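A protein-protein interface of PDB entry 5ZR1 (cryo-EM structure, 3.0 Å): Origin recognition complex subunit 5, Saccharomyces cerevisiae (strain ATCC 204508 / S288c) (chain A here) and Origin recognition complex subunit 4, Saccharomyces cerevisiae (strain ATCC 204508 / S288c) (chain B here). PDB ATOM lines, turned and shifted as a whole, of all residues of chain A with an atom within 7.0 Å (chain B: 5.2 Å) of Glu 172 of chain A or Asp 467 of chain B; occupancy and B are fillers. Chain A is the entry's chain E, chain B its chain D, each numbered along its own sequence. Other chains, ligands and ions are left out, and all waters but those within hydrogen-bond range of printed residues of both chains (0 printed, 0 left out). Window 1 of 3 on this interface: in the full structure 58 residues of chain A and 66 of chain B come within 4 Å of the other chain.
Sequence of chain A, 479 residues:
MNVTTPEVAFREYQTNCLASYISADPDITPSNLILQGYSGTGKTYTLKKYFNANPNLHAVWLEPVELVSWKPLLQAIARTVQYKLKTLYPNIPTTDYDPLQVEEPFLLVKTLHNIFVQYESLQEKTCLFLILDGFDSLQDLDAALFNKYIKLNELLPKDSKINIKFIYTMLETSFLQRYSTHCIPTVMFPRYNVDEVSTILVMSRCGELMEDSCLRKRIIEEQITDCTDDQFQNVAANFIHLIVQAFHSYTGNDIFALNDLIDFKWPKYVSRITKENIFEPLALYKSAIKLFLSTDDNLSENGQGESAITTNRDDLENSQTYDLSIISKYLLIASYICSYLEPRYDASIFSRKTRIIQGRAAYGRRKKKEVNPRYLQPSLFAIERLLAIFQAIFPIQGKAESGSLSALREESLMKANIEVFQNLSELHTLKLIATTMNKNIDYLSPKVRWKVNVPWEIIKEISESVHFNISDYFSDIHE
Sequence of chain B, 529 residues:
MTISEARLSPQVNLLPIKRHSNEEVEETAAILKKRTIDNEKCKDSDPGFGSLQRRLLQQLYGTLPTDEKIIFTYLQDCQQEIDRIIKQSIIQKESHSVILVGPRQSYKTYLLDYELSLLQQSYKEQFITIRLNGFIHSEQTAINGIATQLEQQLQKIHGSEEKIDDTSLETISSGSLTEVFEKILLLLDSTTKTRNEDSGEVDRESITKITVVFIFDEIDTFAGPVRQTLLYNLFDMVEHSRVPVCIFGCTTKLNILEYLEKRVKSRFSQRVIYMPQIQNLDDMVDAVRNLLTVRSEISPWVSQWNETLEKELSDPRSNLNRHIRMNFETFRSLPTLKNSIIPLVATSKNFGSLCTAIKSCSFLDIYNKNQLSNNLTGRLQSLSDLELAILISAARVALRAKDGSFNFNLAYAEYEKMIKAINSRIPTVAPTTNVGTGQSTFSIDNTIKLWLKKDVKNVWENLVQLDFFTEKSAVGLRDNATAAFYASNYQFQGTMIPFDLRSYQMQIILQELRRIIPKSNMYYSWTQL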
ATOM      1  N   GLN A  36     -11.303   0.432  15.458  1.00  0.00           N
ATOM      2  CA  GLN A  36     -10.476  -0.521  16.177  1.00  0.00           C
ATOM      3  C   GLN A  36      -9.325   0.193  16.870  1.00  0.00           C
ATOM      4  O   GLN A  36      -8.565   0.917  16.227  1.00  0.00           O
ATOM      5  CB  GLN A  36      -9.870  -1.593  15.277  1.00  0.00           C
ATOM      6  CG  GLN A  36      -9.214  -2.576  16.192  1.00  0.00           C
ATOM      7  CD  GLN A  36      -7.947  -3.152  15.696  1.00  0.00           C
ATOM      8  OE1 GLN A  36      -7.638  -3.127  14.515  1.00  0.00           O
ATOM      9  NE2 GLN A  36      -7.104  -3.501  16.644  1.00  0.00           N
ATOM     10  N   GLY A  37      -9.185  -0.028  18.170  1.00  0.00           N
ATOM     11  CA  GLY A  37      -7.926   0.251  18.831  1.00  0.00           C
ATOM     12  C   GLY A  37      -7.872  -0.567  20.096  1.00  0.00           C
ATOM     13  O   GLY A  37      -8.877  -1.115  20.540  1.00  0.00           O
ATOM     14  N   TYR A  38      -6.693  -0.640  20.693  1.00  0.00           N
ATOM     15  CA  TYR A  38      -6.561  -1.347  21.958  1.00  0.00           C
ATOM     16  C   TYR A  38      -7.054  -0.471  23.106  1.00  0.00           C
ATOM     17  O   TYR A  38      -7.637   0.598  22.906  1.00  0.00           O
ATOM     18  CB  TYR A  38      -5.131  -1.836  22.136  1.00  0.00           C
ATOM     19  CG  TYR A  38      -4.914  -3.117  21.393  1.00  0.00           C
ATOM     20  CD1 TYR A  38      -5.224  -4.328  21.989  1.00  0.00           C
ATOM     21  CD2 TYR A  38      -4.474  -3.122  20.079  1.00  0.00           C
ATOM     22  CE1 TYR A  38      -5.059  -5.509  21.321  1.00  0.00           C
ATOM     23  CE2 TYR A  38      -4.314  -4.303  19.398  1.00  0.00           C
ATOM     24  CZ  TYR A  38      -4.602  -5.492  20.028  1.00  0.00           C
ATOM     25  OH  TYR A  38      -4.441  -6.678  19.366  1.00  0.00           O
ATOM     26  N   ASP A 136     -16.406  -6.306  20.811  1.00  0.00           N
ATOM     27  CA  ASP A 136     -15.521  -7.430  21.075  1.00  0.00           C
ATOM     28  C   ASP A 136     -15.474  -7.802  22.551  1.00  0.00           C
ATOM     29  O   ASP A 136     -15.153  -8.948  22.881  1.00  0.00           O
ATOM     30  CB  ASP A 136     -14.127  -7.094  20.538  1.00  0.00           C
ATOM     31  CG  ASP A 136     -13.153  -8.232  20.683  1.00  0.00           C
ATOM     32  OD1 ASP A 136     -13.364  -9.280  20.045  1.00  0.00           O
ATOM     33  OD2 ASP A 136     -12.155  -8.064  21.410  1.00  0.00           O
ATOM     34  N   LEU A 141     -18.781 -14.200  23.139  1.00  0.00           N
ATOM     35  CA  LEU A 141     -18.618 -13.870  21.735  1.00  0.00           C
ATOM     36  C   LEU A 141     -18.070 -15.055  20.950  1.00  0.00           C
ATOM     37  O   LEU A 141     -17.294 -15.865  21.458  1.00  0.00           O
ATOM     38  CB  LEU A 141     -17.685 -12.673  21.601  1.00  0.00           C
ATOM     39  CG  LEU A 141     -17.538 -11.986  20.256  1.00  0.00           C
ATOM     40  CD1 LEU A 141     -18.851 -11.355  19.851  1.00  0.00           C
ATOM     41  CD2 LEU A 141     -16.461 -10.956  20.383  1.00  0.00           C
ATOM     42  N   MET A 170     -13.974  -1.998  18.773  1.00  0.00           N
ATOM     43  CA  MET A 170     -13.430  -3.299  19.128  1.00  0.00           C
ATOM     44  C   MET A 170     -11.928  -3.197  19.327  1.00  0.00           C
ATOM     45  O   MET A 170     -11.294  -2.224  18.922  1.00  0.00           O
ATOM     46  CB  MET A 170     -13.789  -4.358  18.081  1.00  0.00           C
ATOM     47  CG  MET A 170     -13.351  -4.058  16.681  1.00  0.00           C
ATOM     48  SD  MET A 170     -14.015  -5.305  15.564  1.00  0.00           S
ATOM     49  CE  MET A 170     -15.767  -4.957  15.673  1.00  0.00           C
ATOM     50  N   LEU A 171     -11.367  -4.220  19.969  1.00  0.00           N
ATOM     51  CA  LEU A 171     -10.038  -4.127  20.562  1.00  0.00           C
ATOM     52  C   LEU A 171      -8.953  -4.883  19.803  1.00  0.00           C
ATOM     53  O   LEU A 171      -7.964  -4.281  19.378  1.00  0.00           O
ATOM     54  CB  LEU A 171     -10.098  -4.631  22.011  1.00  0.00           C
ATOM     55  CG  LEU A 171     -10.753  -3.746  23.068  1.00  0.00           C
ATOM     56  CD1 LEU A 171     -11.104  -4.564  24.274  1.00  0.00           C
ATOM     57  CD2 LEU A 171      -9.795  -2.672  23.483  1.00  0.00           C
ATOM     58  N   GLU A 172      -9.122  -6.185  19.609  1.00  0.00           N
ATOM     59  CA  GLU A 172      -7.987  -7.091  19.711  1.00  0.00           C
ATOM     60  C   GLU A 172      -7.353  -7.519  18.392  1.00  0.00           C
ATOM     61  O   GLU A 172      -6.462  -8.369  18.427  1.00  0.00           O
ATOM     62  CB  GLU A 172      -8.401  -8.332  20.504  1.00  0.00           C
ATOM     63  CG  GLU A 172      -9.466  -9.171  19.846  1.00  0.00           C
ATOM     64  CD  GLU A 172      -9.934 -10.302  20.740  1.00  0.00           C
ATOM     65  OE1 GLU A 172      -9.432 -10.402  21.879  1.00  0.00           O
ATOM     66  OE2 GLU A 172     -10.806 -11.090  20.310  1.00  0.00           O
ATOM     67  N   THR A 173      -7.852  -7.051  17.239  1.00  0.00           N
ATOM     68  CA  THR A 173      -7.305  -7.144  15.870  1.00  0.00           C
ATOM     69  C   THR A 173      -7.119  -8.557  15.329  1.00  0.00           C
ATOM     70  O   THR A 173      -6.826  -8.724  14.146  1.00  0.00           O
ATOM     71  CB  THR A 173      -5.968  -6.390  15.677  1.00  0.00           C
ATOM     72  OG1 THR A 173      -5.807  -6.109  14.283  1.00  0.00           O
ATOM     73  CG2 THR A 173      -4.734  -7.179  16.074  1.00  0.00           C
ATOM     74  N   SER A 174      -7.323  -9.578  16.148  1.00  0.00           N
ATOM     75  CA  SER A 174      -7.494 -10.926  15.643  1.00  0.00           C
ATOM     76  C   SER A 174      -8.962 -11.224  15.442  1.00  0.00           C
ATOM     77  O   SER A 174      -9.319 -12.054  14.600  1.00  0.00           O
ATOM     78  CB  SER A 174      -6.879 -11.936  16.609  1.00  0.00           C
ATOM     79  OG  SER A 174      -7.573 -11.928  17.841  1.00  0.00           O
ATOM     80  N   PHE A 175      -9.811 -10.543  16.207  1.00  0.00           N
ATOM     81  CA  PHE A 175     -11.240 -10.545  15.939  1.00  0.00           C
ATOM     82  C   PHE A 175     -11.558  -9.790  14.658  1.00  0.00           C
ATOM     83  O   PHE A 175     -12.468 -10.172  13.918  1.00  0.00           O
ATOM     84  CB  PHE A 175     -11.977  -9.930  17.124  1.00  0.00           C
ATOM     85  CG  PHE A 175     -13.463  -9.872  16.953  1.00  0.00           C
ATOM     86  CD1 PHE A 175     -14.225 -11.013  17.052  1.00  0.00           C
ATOM     87  CD2 PHE A 175     -14.097  -8.670  16.713  1.00  0.00           C
ATOM     88  CE1 PHE A 175     -15.587 -10.965  16.901  1.00  0.00           C
ATOM     89  CE2 PHE A 175     -15.464  -8.614  16.561  1.00  0.00           C
ATOM     90  CZ  PHE A 175     -16.209  -9.763  16.658  1.00  0.00           C
ATOM     91  N   LEU A 176     -10.818  -8.720  14.377  1.00  0.00           N
ATOM     92  CA  LEU A 176     -11.121  -7.902  13.212  1.00  0.00           C
ATOM     93  C   LEU A 176     -10.676  -8.570  11.918  1.00  0.00           C
ATOM     94  O   LEU A 176     -11.342  -8.430  10.888  1.00  0.00           O
ATOM     95  CB  LEU A 176     -10.466  -6.531  13.360  1.00  0.00           C
ATOM     96  CG  LEU A 176     -10.771  -5.526  12.257  1.00  0.00           C
ATOM     97  CD1 LEU A 176     -12.242  -5.186  12.260  1.00  0.00           C
ATOM     98  CD2 LEU A 176      -9.922  -4.290  12.401  1.00  0.00           C
ATOM     99  N   ARG A 178     -10.853 -11.600  11.091  1.00  0.00           N
ATOM    100  CA  ARG A 178     -11.777 -12.623  10.628  1.00  0.00           C
ATOM    101  C   ARG A 178     -12.786 -12.079   9.632  1.00  0.00           C
ATOM    102  O   ARG A 178     -13.435 -12.862   8.936  1.00  0.00           O
ATOM    103  CB  ARG A 178     -12.521 -13.239  11.805  1.00  0.00           C
ATOM    104  CG  ARG A 178     -11.686 -14.117  12.691  1.00  0.00           C
ATOM    105  CD  ARG A 178     -12.534 -14.704  13.798  1.00  0.00           C
ATOM    106  NE  ARG A 178     -11.794 -15.680  14.587  1.00  0.00           N
ATOM    107  CZ  ARG A 178     -11.072 -15.378  15.658  1.00  0.00           C
ATOM    108  NH1 ARG A 178     -10.428 -16.331  16.315  1.00  0.00           N
ATOM    109  NH2 ARG A 178     -10.985 -14.124  16.069  1.00  0.00           N
ATOM    110  N   LEU B 376       0.850  -6.251  13.872  1.00  0.00           N
ATOM    111  CA  LEU B 376       1.823  -6.835  14.791  1.00  0.00           C
ATOM    112  C   LEU B 376       3.157  -6.109  14.786  1.00  0.00           C
ATOM    113  O   LEU B 376       3.876  -6.165  15.787  1.00  0.00           O
ATOM    114  CB  LEU B 376       2.037  -8.322  14.477  1.00  0.00           C
ATOM    115  CG  LEU B 376       2.772  -9.215  15.480  1.00  0.00           C
ATOM    116  CD1 LEU B 376       2.061  -9.190  16.816  1.00  0.00           C
ATOM    117  CD2 LEU B 376       2.845 -10.636  14.962  1.00  0.00           C
ATOM    118  N   ARG B 379       2.362  -2.838  16.947  1.00  0.00           N
ATOM    119  CA  ARG B 379       2.292  -3.071  18.384  1.00  0.00           C
ATOM    120  C   ARG B 379       3.671  -3.292  18.982  1.00  0.00           C
ATOM    121  O   ARG B 379       3.922  -2.899  20.126  1.00  0.00           O
ATOM    122  CB  ARG B 379       1.394  -4.265  18.696  1.00  0.00           C
ATOM    123  CG  ARG B 379      -0.070  -3.969  18.579  1.00  0.00           C
ATOM    124  CD  ARG B 379      -0.903  -5.171  18.930  1.00  0.00           C
ATOM    125  NE  ARG B 379      -0.795  -6.229  17.938  1.00  0.00           N
ATOM    126  CZ  ARG B 379      -1.418  -7.396  18.029  1.00  0.00           C
ATOM    127  NH1 ARG B 379      -2.207  -7.645  19.054  1.00  0.00           N
ATOM    128  NH2 ARG B 379      -1.267  -8.303  17.080  1.00  0.00           N
ATOM    129  N   LEU B 463       1.390  -8.168  27.685  1.00  0.00           N
ATOM    130  CA  LEU B 463       1.780  -8.909  26.497  1.00  0.00           C
ATOM    131  C   LEU B 463       0.813 -10.038  26.190  1.00  0.00           C
ATOM    132  O   LEU B 463       0.752 -10.494  25.047  1.00  0.00           O
ATOM    133  CB  LEU B 463       3.187  -9.464  26.679  1.00  0.00           C
ATOM    134  CG  LEU B 463       4.279  -8.420  26.876  1.00  0.00           C
ATOM    135  CD1 LEU B 463       5.577  -9.100  27.215  1.00  0.00           C
ATOM    136  CD2 LEU B 463       4.434  -7.562  25.641  1.00  0.00           C
ATOM    137  N   VAL B 464       0.076 -10.512  27.194  1.00  0.00           N
ATOM    138  CA  VAL B 464      -1.006 -11.457  26.950  1.00  0.00           C
ATOM    139  C   VAL B 464      -2.160 -10.767  26.233  1.00  0.00           C
ATOM    140  O   VAL B 464      -2.679 -11.272  25.232  1.00  0.00           O
ATOM    141  CB  VAL B 464      -1.461 -12.097  28.273  1.00  0.00           C
ATOM    142  CG1 VAL B 464      -2.710 -12.922  28.069  1.00  0.00           C
ATOM    143  CG2 VAL B 464      -0.368 -12.976  28.821  1.00  0.00           C
ATOM    144  N   GLN B 465      -2.562  -9.588  26.711  1.00  0.00           N
ATOM    145  CA  GLN B 465      -3.744  -8.952  26.146  1.00  0.00           C
ATOM    146  C   GLN B 465      -3.463  -8.167  24.874  1.00  0.00           C
ATOM    147  O   GLN B 465      -4.410  -7.675  24.255  1.00  0.00           O
ATOM    148  CB  GLN B 465      -4.408  -8.027  27.165  1.00  0.00           C
ATOM    149  CG  GLN B 465      -3.645  -6.771  27.475  1.00  0.00           C
ATOM    150  CD  GLN B 465      -4.420  -5.866  28.408  1.00  0.00           C
ATOM    151  OE1 GLN B 465      -5.551  -6.170  28.780  1.00  0.00           O
ATOM    152  NE2 GLN B 465      -3.821  -4.742  28.780  1.00  0.00           N
ATOM    153  N   LEU B 466      -2.204  -8.033  24.466  1.00  0.00           N
ATOM    154  CA  LEU B 466      -1.860  -7.438  23.182  1.00  0.00           C
ATOM    155  C   LEU B 466      -1.577  -8.475  22.111  1.00  0.00           C
ATOM    156  O   LEU B 466      -1.054  -8.109  21.055  1.00  0.00           O
ATOM    157  CB  LEU B 466      -0.647  -6.517  23.319  1.00  0.00           C
ATOM    158  CG  LEU B 466      -0.834  -5.185  24.032  1.00  0.00           C
ATOM    159  CD1 LEU B 466       0.506  -4.518  24.243  1.00  0.00           C
ATOM    160  CD2 LEU B 466      -1.740  -4.297  23.220  1.00  0.00           C
ATOM    161  N   ASP B 467      -1.919  -9.743  22.361  1.00  0.00           N
ATOM    162  CA  ASP B 467      -1.656 -10.877  21.465  1.00  0.00           C
ATOM    163  C   ASP B 467      -0.185 -10.968  21.067  1.00  0.00           C
ATOM    164  O   ASP B 467       0.169 -10.955  19.888  1.00  0.00           O
ATOM    165  CB  ASP B 467      -2.550 -10.841  20.223  1.00  0.00           C
ATOM    166  CG  ASP B 467      -3.962 -11.307  20.503  1.00  0.00           C
ATOM    167  OD1 ASP B 467      -4.142 -12.154  21.402  1.00  0.00           O
ATOM    168  OD2 ASP B 467      -4.892 -10.839  19.813  1.00  0.00           O
ATOM    169  N   PHE B 468       0.680 -11.013  22.070  1.00  0.00           N
ATOM    170  CA  PHE B 468       2.038 -11.488  21.871  1.00  0.00           C
ATOM    171  C   PHE B 468       2.239 -12.874  22.444  1.00  0.00           C
ATOM    172  O   PHE B 468       3.060 -13.639  21.932  1.00  0.00           O
ATOM    173  CB  PHE B 468       3.047 -10.530  22.505  1.00  0.00           C
ATOM    174  CG  PHE B 468       3.177  -9.221  21.791  1.00  0.00           C
ATOM    175  CD1 PHE B 468       3.902  -9.133  20.617  1.00  0.00           C
ATOM    176  CD2 PHE B 468       2.599  -8.076  22.303  1.00  0.00           C
ATOM    177  CE1 PHE B 468       4.030  -7.934  19.959  1.00  0.00           C
ATOM    178  CE2 PHE B 468       2.725  -6.874  21.647  1.00  0.00           C
ATOM    179  CZ  PHE B 468       3.445  -6.803  20.477  1.00  0.00           C
ATOM    180  N   PHE B 469       1.496 -13.201  23.495  1.00  0.00           N
ATOM    181  CA  PHE B 469       1.495 -14.509  24.127  1.00  0.00           C
ATOM    182  C   PHE B 469       0.088 -15.062  24.020  1.00  0.00           C
ATOM    183  O   PHE B 469      -0.885 -14.338  24.245  1.00  0.00           O
ATOM    184  CB  PHE B 469       1.864 -14.431  25.614  1.00  0.00           C
ATOM    185  CG  PHE B 469       3.227 -13.872  25.896  1.00  0.00           C
ATOM    186  CD1 PHE B 469       4.243 -13.916  24.959  1.00  0.00           C
ATOM    187  CD2 PHE B 469       3.472 -13.263  27.109  1.00  0.00           C
ATOM    188  CE1 PHE B 469       5.476 -13.377  25.234  1.00  0.00           C
ATOM    189  CE2 PHE B 469       4.702 -12.724  27.387  1.00  0.00           C
ATOM    190  CZ  PHE B 469       5.703 -12.783  26.448  1.00  0.00           C
ATOM    191  N   THR B 470      -0.034 -16.332  23.679  1.00  0.00           N
ATOM    192  CA  THR B 470      -1.319 -16.998  23.754  1.00  0.00           C
ATOM    193  C   THR B 470      -1.225 -18.148  24.738  1.00  0.00           C
ATOM    194  O   THR B 470      -0.144 -18.669  25.009  1.00  0.00           O
ATOM    195  CB  THR B 470      -1.780 -17.517  22.389  1.00  0.00           C
ATOM    196  OG1 THR B 470      -0.789 -18.394  21.846  1.00  0.00           O
ATOM    197  CG2 THR B 470      -2.027 -16.370  21.441  1.00  0.00           C
ATOM    198  N   LEU B 477     -11.892 -18.053  19.608  1.00  0.00           N
ATOM    199  CA  LEU B 477     -13.308 -17.920  19.318  1.00  0.00           C
ATOM    200  C   LEU B 477     -13.802 -19.186  18.652  1.00  0.00           C
ATOM    201  O   LEU B 477     -13.095 -19.789  17.841  1.00  0.00           O
ATOM    202  CB  LEU B 477     -13.609 -16.736  18.410  1.00  0.00           C
ATOM    203  CG  LEU B 477     -13.450 -15.329  18.945  1.00  0.00           C
ATOM    204  CD1 LEU B 477     -13.859 -14.431  17.833  1.00  0.00           C
ATOM    205  CD2 LEU B 477     -14.315 -15.115  20.160  1.00  0.00           C
ATOM    206  N   GLN B 507       3.361 -15.597  19.653  1.00  0.00           N
ATOM    207  CA  GLN B 507       2.822 -15.053  18.411  1.00  0.00           C
ATOM    208  C   GLN B 507       3.928 -14.693  17.431  1.00  0.00           C
ATOM    209  O   GLN B 507       3.821 -14.976  16.232  1.00  0.00           O
ATOM    210  CB  GLN B 507       1.972 -13.827  18.716  1.00  0.00           C
ATOM    211  CG  GLN B 507       0.630 -14.120  19.332  1.00  0.00           C
ATOM    212  CD  GLN B 507      -0.326 -14.710  18.337  1.00  0.00           C
ATOM    213  OE1 GLN B 507      -0.722 -15.857  18.451  1.00  0.00           O
ATOM    214  NE2 GLN B 507      -0.688 -13.927  17.335  1.00  0.00           N
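The guanidinium group (NH1) of Arg 379 of chain B lies within hydrogen-bond range of the side-chain hydroxyl (OH) of Tyr 38 of chain A, 2.5 Å away. The backbone carbonyl oxygen (O) of Glu 172 of chain A sits close to the side-chain carboxylate (OD2) of Asp 467 of chain B (3.2 Å).
The backbone carbonyl oxygen (O) of Glu 172 of chain A sits at hydrogen-bond distance from the side-chain hydroxyl (OH) of Tyr 38 of chain A (2.8 Å). The guanidinium group of Arg 178 of chain A sits at hydrogen-bond distance from the backbone carbonyl oxygen of Ser 174 of chain A (3.0 Å).
Among the printed residues, merely in contact across the chains: Tyr 38 of chain A with Gln 465 of chain B, Tyr 38 of chain A with Leu 466 of chain B, Leu 141 of chain A with Leu 477 of chain B, Thr 173 of chain A with Arg 379 of chain B, Ser 174 of chain A with Asp 467 of chain B, Phe 175 of chain A with Leu 477 of chain B and Arg 178 of chain A with Leu 477 of chain B.
Of chain B, only Asp 467 comes within 4 Å of Glu 172 of chain A. Printed residues of chain A within 4 Å of Gln 465 of chain B: Tyr 38. Asp 467 of chain B touches just these residues of chain A: Glu 172 and Ser 174. Of the printed residues of chain A, Leu 477 of chain B touches Leu 141, Phe 175 and Arg 178. The nearest residue of chain A that does not touch Asp 467 of chain B is Tyr 38 of chain A (4.2 Å). The nearest printed residue of chain A that does not touch Leu 466 of chain B is Glu 172 of chain A (6.0 Å).
Printed residues of chain A that touch a printed residue of chain B: Tyr 38, Leu 141, Glu 172, Thr 173, Ser 174, Phe 175 and Arg 178. Hydrophobic or aromatic side chains of chain A within 4 Å of the printed part of chain B: Tyr 38 and Phe 175. Printed residues of chain B that touch a printed residue of chain A: Arg 379, Gln 465, Leu 466, Asp 467 and Leu 477.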
